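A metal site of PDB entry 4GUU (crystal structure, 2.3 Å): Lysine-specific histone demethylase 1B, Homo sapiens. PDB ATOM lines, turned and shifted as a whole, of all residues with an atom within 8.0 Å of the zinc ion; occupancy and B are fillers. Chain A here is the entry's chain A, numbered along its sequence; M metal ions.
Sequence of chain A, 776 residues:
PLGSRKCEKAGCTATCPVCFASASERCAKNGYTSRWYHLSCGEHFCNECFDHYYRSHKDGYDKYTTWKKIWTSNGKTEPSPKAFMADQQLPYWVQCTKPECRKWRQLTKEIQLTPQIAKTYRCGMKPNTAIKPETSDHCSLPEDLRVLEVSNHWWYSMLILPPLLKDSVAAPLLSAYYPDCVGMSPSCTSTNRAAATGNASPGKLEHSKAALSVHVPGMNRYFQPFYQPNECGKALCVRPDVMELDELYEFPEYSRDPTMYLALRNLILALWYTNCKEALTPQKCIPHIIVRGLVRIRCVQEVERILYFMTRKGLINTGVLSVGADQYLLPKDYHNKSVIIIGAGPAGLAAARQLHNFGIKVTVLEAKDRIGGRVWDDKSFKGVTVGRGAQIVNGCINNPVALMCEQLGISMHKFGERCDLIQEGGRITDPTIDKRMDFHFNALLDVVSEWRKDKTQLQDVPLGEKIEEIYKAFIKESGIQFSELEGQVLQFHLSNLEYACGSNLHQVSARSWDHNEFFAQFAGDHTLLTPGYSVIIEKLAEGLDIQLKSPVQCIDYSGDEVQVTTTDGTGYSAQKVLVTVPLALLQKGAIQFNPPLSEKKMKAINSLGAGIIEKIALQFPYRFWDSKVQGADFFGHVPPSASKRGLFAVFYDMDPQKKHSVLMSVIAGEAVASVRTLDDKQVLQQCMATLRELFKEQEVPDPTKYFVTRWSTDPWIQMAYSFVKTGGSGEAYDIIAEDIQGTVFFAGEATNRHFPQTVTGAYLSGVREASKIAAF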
ATOM      1  N   LYS A   6       8.465 -22.134 -23.082  1.00  0.00           N
ATOM      2  CA  LYS A   6       7.985 -21.835 -24.425  1.00  0.00           C
ATOM      3  C   LYS A   6       7.602 -20.368 -24.570  1.00  0.00           C
ATOM      4  O   LYS A   6       7.143 -19.736 -23.619  1.00  0.00           O
ATOM      5  CB  LYS A   6       6.796 -22.728 -24.776  1.00  0.00           C
ATOM      6  CG  LYS A   6       7.168 -23.900 -25.671  1.00  0.00           C
ATOM      7  CD  LYS A   6       7.715 -23.399 -26.991  1.00  0.00           C
ATOM      8  CE  LYS A   6       8.594 -24.432 -27.668  1.00  0.00           C
ATOM      9  NZ  LYS A   6       9.145 -23.925 -28.953  1.00  0.00           N
ATOM     10  N   CYS A   7       7.808 -19.828 -25.769  1.00  0.00           N
ATOM     11  CA  CYS A   7       7.532 -18.425 -26.032  1.00  0.00           C
ATOM     12  C   CYS A   7       6.047 -18.138 -26.265  1.00  0.00           C
ATOM     13  O   CYS A   7       5.389 -18.831 -27.040  1.00  0.00           O
ATOM     14  CB  CYS A   7       8.344 -17.915 -27.217  1.00  0.00           C
ATOM     15  SG  CYS A   7       7.793 -16.296 -27.778  1.00  0.00           S
ATOM     16  N   GLU A   8       5.540 -17.104 -25.603  1.00  0.00           N
ATOM     17  CA  GLU A   8       4.176 -16.636 -25.813  1.00  0.00           C
ATOM     18  C   GLU A   8       3.819 -16.604 -27.296  1.00  0.00           C
ATOM     19  O   GLU A   8       2.750 -17.066 -27.695  1.00  0.00           O
ATOM     20  CB  GLU A   8       4.031 -15.229 -25.246  1.00  0.00           C
ATOM     21  CG  GLU A   8       4.935 -14.205 -25.918  1.00  0.00           C
ATOM     22  CD  GLU A   8       4.724 -12.795 -25.398  1.00  0.00           C
ATOM     23  OE1 GLU A   8       5.504 -11.901 -25.785  1.00  0.00           O
ATOM     24  OE2 GLU A   8       3.792 -12.592 -24.595  1.00  0.00           O
ATOM     25  N   LYS A   9       4.727 -16.059 -28.102  1.00  0.00           N
ATOM     26  CA  LYS A   9       4.501 -15.836 -29.518  1.00  0.00           C
ATOM     27  C   LYS A   9       4.285 -17.119 -30.304  1.00  0.00           C
ATOM     28  O   LYS A   9       5.156 -17.981 -30.360  1.00  0.00           O
ATOM     29  CB  LYS A   9       5.679 -15.061 -30.111  1.00  0.00           C
ATOM     30  CG  LYS A   9       5.626 -14.847 -31.616  1.00  0.00           C
ATOM     31  CD  LYS A   9       4.652 -13.748 -31.992  1.00  0.00           C
ATOM     32  CE  LYS A   9       5.093 -13.048 -33.258  1.00  0.00           C
ATOM     33  NZ  LYS A   9       4.083 -12.077 -33.769  1.00  0.00           N
ATOM     34  N   ALA A  10       3.101 -17.236 -30.908  1.00  0.00           N
ATOM     35  CA  ALA A  10       2.815 -18.347 -31.793  1.00  0.00           C
ATOM     36  C   ALA A  10       3.690 -18.239 -33.036  1.00  0.00           C
ATOM     37  O   ALA A  10       3.805 -17.170 -33.626  1.00  0.00           O
ATOM     38  CB  ALA A  10       1.342 -18.349 -32.178  1.00  0.00           C
ATOM     39  N   GLY A  11       4.326 -19.343 -33.409  1.00  0.00           N
ATOM     40  CA  GLY A  11       5.166 -19.356 -34.597  1.00  0.00           C
ATOM     41  C   GLY A  11       6.617 -19.028 -34.339  1.00  0.00           C
ATOM     42  O   GLY A  11       7.464 -19.241 -35.195  1.00  0.00           O
ATOM     43  N   CYS A  12       6.925 -18.508 -33.148  1.00  0.00           N
ATOM     44  CA  CYS A  12       8.317 -18.221 -32.819  1.00  0.00           C
ATOM     45  C   CYS A  12       9.171 -19.478 -32.860  1.00  0.00           C
ATOM     46  O   CYS A  12       8.722 -20.561 -32.499  1.00  0.00           O
ATOM     47  CB  CYS A  12       8.450 -17.555 -31.447  1.00  0.00           C
ATOM     48  SG  CYS A  12      10.187 -17.406 -30.950  1.00  0.00           S
ATOM     49  N   THR A  13      10.420 -19.314 -33.298  1.00  0.00           N
ATOM     50  CA  THR A  13      11.301 -20.446 -33.543  1.00  0.00           C
ATOM     51  C   THR A  13      12.219 -20.753 -32.360  1.00  0.00           C
ATOM     52  O   THR A  13      12.871 -21.787 -32.340  1.00  0.00           O
ATOM     53  CB  THR A  13      12.174 -20.210 -34.787  1.00  0.00           C
ATOM     54  OG1 THR A  13      13.340 -19.458 -34.421  1.00  0.00           O
ATOM     55  CG2 THR A  13      11.384 -19.437 -35.834  1.00  0.00           C
ATOM     56  N   ALA A  14      12.259 -19.852 -31.384  1.00  0.00           N
ATOM     57  CA  ALA A  14      13.128 -20.051 -30.239  1.00  0.00           C
ATOM     58  C   ALA A  14      12.746 -21.272 -29.406  1.00  0.00           C
ATOM     59  O   ALA A  14      11.736 -21.265 -28.695  1.00  0.00           O
ATOM     60  CB  ALA A  14      13.145 -18.810 -29.369  1.00  0.00           C
ATOM     61  N   THR A  15      13.570 -22.314 -29.461  1.00  0.00           N
ATOM     62  CA  THR A  15      13.326 -23.542 -28.719  1.00  0.00           C
ATOM     63  C   THR A  15      13.696 -23.392 -27.253  1.00  0.00           C
ATOM     64  O   THR A  15      13.090 -24.041 -26.389  1.00  0.00           O
ATOM     65  CB  THR A  15      14.090 -24.742 -29.321  1.00  0.00           C
ATOM     66  OG1 THR A  15      15.452 -24.375 -29.574  1.00  0.00           O
ATOM     67  CG2 THR A  15      13.440 -25.187 -30.621  1.00  0.00           C
ATOM     68  N   PRO A  17      14.126 -20.203 -24.904  1.00  0.00           N
ATOM     69  CA  PRO A  17      14.155 -18.790 -24.534  1.00  0.00           C
ATOM     70  C   PRO A  17      15.061 -18.575 -23.334  1.00  0.00           C
ATOM     71  O   PRO A  17      15.043 -19.390 -22.406  1.00  0.00           O
ATOM     72  CB  PRO A  17      12.703 -18.495 -24.141  1.00  0.00           C
ATOM     73  CG  PRO A  17      11.899 -19.549 -24.817  1.00  0.00           C
ATOM     74  CD  PRO A  17      12.766 -20.760 -24.824  1.00  0.00           C
ATOM     75  N   TRP A  36       7.020 -16.037 -21.139  1.00  0.00           N
ATOM     76  CA  TRP A  36       8.173 -15.489 -21.861  1.00  0.00           C
ATOM     77  C   TRP A  36       7.730 -14.430 -22.843  1.00  0.00           C
ATOM     78  O   TRP A  36       6.852 -14.675 -23.671  1.00  0.00           O
ATOM     79  CB  TRP A  36       8.917 -16.597 -22.597  1.00  0.00           C
ATOM     80  CG  TRP A  36       9.861 -17.388 -21.746  1.00  0.00           C
ATOM     81  CD1 TRP A  36       9.702 -18.678 -21.343  1.00  0.00           C
ATOM     82  CD2 TRP A  36      11.095 -16.928 -21.181  1.00  0.00           C
ATOM     83  NE1 TRP A  36      10.772 -19.059 -20.559  1.00  0.00           N
ATOM     84  CE2 TRP A  36      11.638 -18.009 -20.448  1.00  0.00           C
ATOM     85  CE3 TRP A  36      11.790 -15.714 -21.224  1.00  0.00           C
ATOM     86  CZ2 TRP A  36      12.851 -17.902 -19.763  1.00  0.00           C
ATOM     87  CZ3 TRP A  36      12.991 -15.615 -20.540  1.00  0.00           C
ATOM     88  CH2 TRP A  36      13.506 -16.702 -19.821  1.00  0.00           C
ATOM     89  N   TYR A  37       8.328 -13.251 -22.761  1.00  0.00           N
ATOM     90  CA  TYR A  37       7.969 -12.156 -23.648  1.00  0.00           C
ATOM     91  C   TYR A  37       8.910 -12.049 -24.831  1.00  0.00           C
ATOM     92  O   TYR A  37      10.129 -12.072 -24.692  1.00  0.00           O
ATOM     93  CB  TYR A  37       7.886 -10.843 -22.867  1.00  0.00           C
ATOM     94  CG  TYR A  37       6.713 -10.819 -21.911  1.00  0.00           C
ATOM     95  CD1 TYR A  37       5.433 -10.497 -22.341  1.00  0.00           C
ATOM     96  CD2 TYR A  37       6.883 -11.141 -20.562  1.00  0.00           C
ATOM     97  CE1 TYR A  37       4.357 -10.481 -21.485  1.00  0.00           C
ATOM     98  CE2 TYR A  37       5.801 -11.128 -19.686  1.00  0.00           C
ATOM     99  CZ  TYR A  37       4.546 -10.805 -20.150  1.00  0.00           C
ATOM    100  OH  TYR A  37       3.476 -10.785 -19.287  1.00  0.00           O
ATOM    101  N   HIS A  38       8.315 -11.934 -26.019  1.00  0.00           N
ATOM    102  CA  HIS A  38       9.037 -12.036 -27.272  1.00  0.00           C
ATOM    103  C   HIS A  38       9.239 -10.700 -27.959  1.00  0.00           C
ATOM    104  O   HIS A  38       8.282 -10.037 -28.349  1.00  0.00           O
ATOM    105  CB  HIS A  38       8.301 -13.003 -28.205  1.00  0.00           C
ATOM    106  CG  HIS A  38       8.731 -12.934 -29.632  1.00  0.00           C
ATOM    107  ND1 HIS A  38       9.247 -14.022 -30.312  1.00  0.00           N
ATOM    108  CD2 HIS A  38       8.698 -11.912 -30.526  1.00  0.00           C
ATOM    109  CE1 HIS A  38       9.518 -13.669 -31.553  1.00  0.00           C
ATOM    110  NE2 HIS A  38       9.192 -12.404 -31.711  1.00  0.00           N
ATOM    111  N   LEU A  39      10.499 -10.290 -28.099  1.00  0.00           N
ATOM    112  CA  LEU A  39      10.852  -9.105 -28.875  1.00  0.00           C
ATOM    113  C   LEU A  39      11.225  -9.540 -30.290  1.00  0.00           C
ATOM    114  O   LEU A  39      10.839  -8.903 -31.272  1.00  0.00           O
ATOM    115  CB  LEU A  39      12.007  -8.356 -28.219  1.00  0.00           C
ATOM    116  CG  LEU A  39      11.665  -7.064 -27.485  1.00  0.00           C
ATOM    117  CD1 LEU A  39      10.203  -7.040 -27.042  1.00  0.00           C
ATOM    118  CD2 LEU A  39      12.596  -6.860 -26.312  1.00  0.00           C
ATOM    119  N   SER A  40      11.972 -10.632 -30.382  1.00  0.00           N
ATOM    120  CA  SER A  40      12.318 -11.246 -31.660  1.00  0.00           C
ATOM    121  C   SER A  40      12.464 -12.747 -31.476  1.00  0.00           C
ATOM    122  O   SER A  40      12.323 -13.256 -30.360  1.00  0.00           O
ATOM    123  CB  SER A  40      13.620 -10.662 -32.212  1.00  0.00           C
ATOM    124  OG  SER A  40      14.740 -11.098 -31.465  1.00  0.00           O
ATOM    125  N   CYS A  41      12.740 -13.455 -32.560  1.00  0.00           N
ATOM    126  CA  CYS A  41      12.961 -14.897 -32.482  1.00  0.00           C
ATOM    127  C   CYS A  41      14.179 -15.253 -31.635  1.00  0.00           C
ATOM    128  O   CYS A  41      14.305 -16.388 -31.169  1.00  0.00           O
ATOM    129  CB  CYS A  41      13.113 -15.488 -33.885  1.00  0.00           C
ATOM    130  SG  CYS A  41      11.573 -15.663 -34.817  1.00  0.00           S
ATOM    131  N   GLY A  42      15.062 -14.288 -31.418  1.00  0.00           N
ATOM    132  CA  GLY A  42      16.277 -14.526 -30.663  1.00  0.00           C
ATOM    133  C   GLY A  42      16.297 -13.836 -29.313  1.00  0.00           C
ATOM    134  O   GLY A  42      17.182 -14.079 -28.491  1.00  0.00           O
ATOM    135  N   GLU A  43      15.316 -12.977 -29.071  1.00  0.00           N
ATOM    136  CA  GLU A  43      15.336 -12.160 -27.864  1.00  0.00           C
ATOM    137  C   GLU A  43      14.038 -12.213 -27.059  1.00  0.00           C
ATOM    138  O   GLU A  43      12.952 -11.934 -27.575  1.00  0.00           O
ATOM    139  CB  GLU A  43      15.688 -10.713 -28.215  1.00  0.00           C
ATOM    140  CG  GLU A  43      17.072 -10.590 -28.835  1.00  0.00           C
ATOM    141  CD  GLU A  43      17.198  -9.419 -29.786  1.00  0.00           C
ATOM    142  OE1 GLU A  43      18.060  -8.557 -29.550  1.00  0.00           O
ATOM    143  OE2 GLU A  43      16.424  -9.369 -30.768  1.00  0.00           O
ATOM    144  N   HIS A  44      14.166 -12.557 -25.789  1.00  0.00           N
ATOM    145  CA  HIS A  44      13.026 -12.669 -24.880  1.00  0.00           C
ATOM    146  C   HIS A  44      13.356 -12.163 -23.488  1.00  0.00           C
ATOM    147  O   HIS A  44      14.530 -12.063 -23.118  1.00  0.00           O
ATOM    148  CB  HIS A  44      12.573 -14.119 -24.782  1.00  0.00           C
ATOM    149  CG  HIS A  44      12.213 -14.741 -26.098  1.00  0.00           C
ATOM    150  ND1 HIS A  44      13.154 -15.271 -26.944  1.00  0.00           N
ATOM    151  CD2 HIS A  44      11.013 -14.914 -26.699  1.00  0.00           C
ATOM    152  CE1 HIS A  44      12.546 -15.751 -28.019  1.00  0.00           C
ATOM    153  NE2 HIS A  44      11.255 -15.548 -27.896  1.00  0.00           N
ATOM    154  N   LYS A  82       7.483  -3.666 -23.762  1.00  0.00           N
ATOM    155  CA  LYS A  82       8.273  -4.239 -24.855  1.00  0.00           C
ATOM    156  C   LYS A  82       9.041  -3.152 -25.595  1.00  0.00           C
ATOM    157  O   LYS A  82      10.161  -3.361 -26.053  1.00  0.00           O
ATOM    158  CB  LYS A  82       7.379  -5.013 -25.829  1.00  0.00           C
ATOM    159  CG  LYS A  82       6.878  -6.357 -25.307  1.00  0.00           C
ATOM    160  CD  LYS A  82       6.533  -7.295 -26.454  1.00  0.00           C
ATOM    161  CE  LYS A  82       5.732  -8.497 -25.971  1.00  0.00           C
ATOM    162  NZ  LYS A  82       5.441  -9.457 -27.078  1.00  0.00           N
ATOM    163  N   MET A 158       8.680 -11.579 -37.507  1.00  0.00           N
ATOM    164  CA  MET A 158       8.584 -12.048 -36.129  1.00  0.00           C
ATOM    165  C   MET A 158       9.089 -11.016 -35.135  1.00  0.00           C
ATOM    166  O   MET A 158       9.118 -11.250 -33.934  1.00  0.00           O
ATOM    167  CB  MET A 158       9.370 -13.349 -35.950  1.00  0.00           C
ATOM    168  CG  MET A 158       8.790 -14.566 -36.668  1.00  0.00           C
ATOM    169  SD  MET A 158       7.478 -15.389 -35.732  1.00  0.00           S
ATOM    170  CE  MET A 158       6.082 -14.320 -36.079  1.00  0.00           C
ATOM    171  N   ILE A 160       8.567  -7.692 -33.200  1.00  0.00           N
ATOM    172  CA  ILE A 160       7.366  -6.994 -32.762  1.00  0.00           C
ATOM    173  C   ILE A 160       7.344  -5.503 -33.109  1.00  0.00           C
ATOM    174  O   ILE A 160       6.412  -5.025 -33.749  1.00  0.00           O
ATOM    175  CB  ILE A 160       7.120  -7.166 -31.254  1.00  0.00           C
ATOM    176  CG1 ILE A 160       6.901  -8.640 -30.921  1.00  0.00           C
ATOM    177  CG2 ILE A 160       5.922  -6.349 -30.815  1.00  0.00           C
ATOM    178  CD1 ILE A 160       5.845  -9.301 -31.791  1.00  0.00           C
HETATM  179 ZN    ZN M   1       9.633 -15.875 -29.292  1.00  0.00          ZN
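The backbone carbonyl oxygen (O) of Ser 40 sits close to a ring nitrogen (ND1) of His 38 (3.2 Å). NE2 of His 38 is in hydrogen-bond range of O of Met 158, at 2.5 Å. SG of Cys 7 sits close to N of Lys 9, 3.1 Å away. The side-chain carboxylate (OE2) of Glu 43 sits at hydrogen-bond distance from the side-chain hydroxyl (OG) of Ser 40. The backbone NH (N) of Gly 42 lies close to the side-chain hydroxyl (OG) of Ser 40. O of His 38 sits at hydrogen-bond distance from NZ of Lys 82. SG of Cys 12 sits close to N of Ala 14, at 3.2 Å. The side-chain carboxylate (OE1) of Glu 8 is in hydrogen-bond range of the backbone NH (N) of His 38 (2.8 Å).
Merely in contact with the zinc ion: Ser 40 (3.9 Å). Of the 23 residues printed, 5 come within 4 Å of the zinc ion. The nearest printed residue that does not touch the zinc ion is Lys 9 (4.1 Å).
The zinc ion is bound by a ring nitrogen (ND1) of His 38 (2.2 Å). NE2 of His 44 binds the zinc ion (2.2 Å). The side-chain sulfur (SG) of Cys 12 binds the zinc ion (2.3 Å). The zinc ion is bound by SG of Cys 7, 2.4 Å away. The zinc ion has four donor atoms within binding distance.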
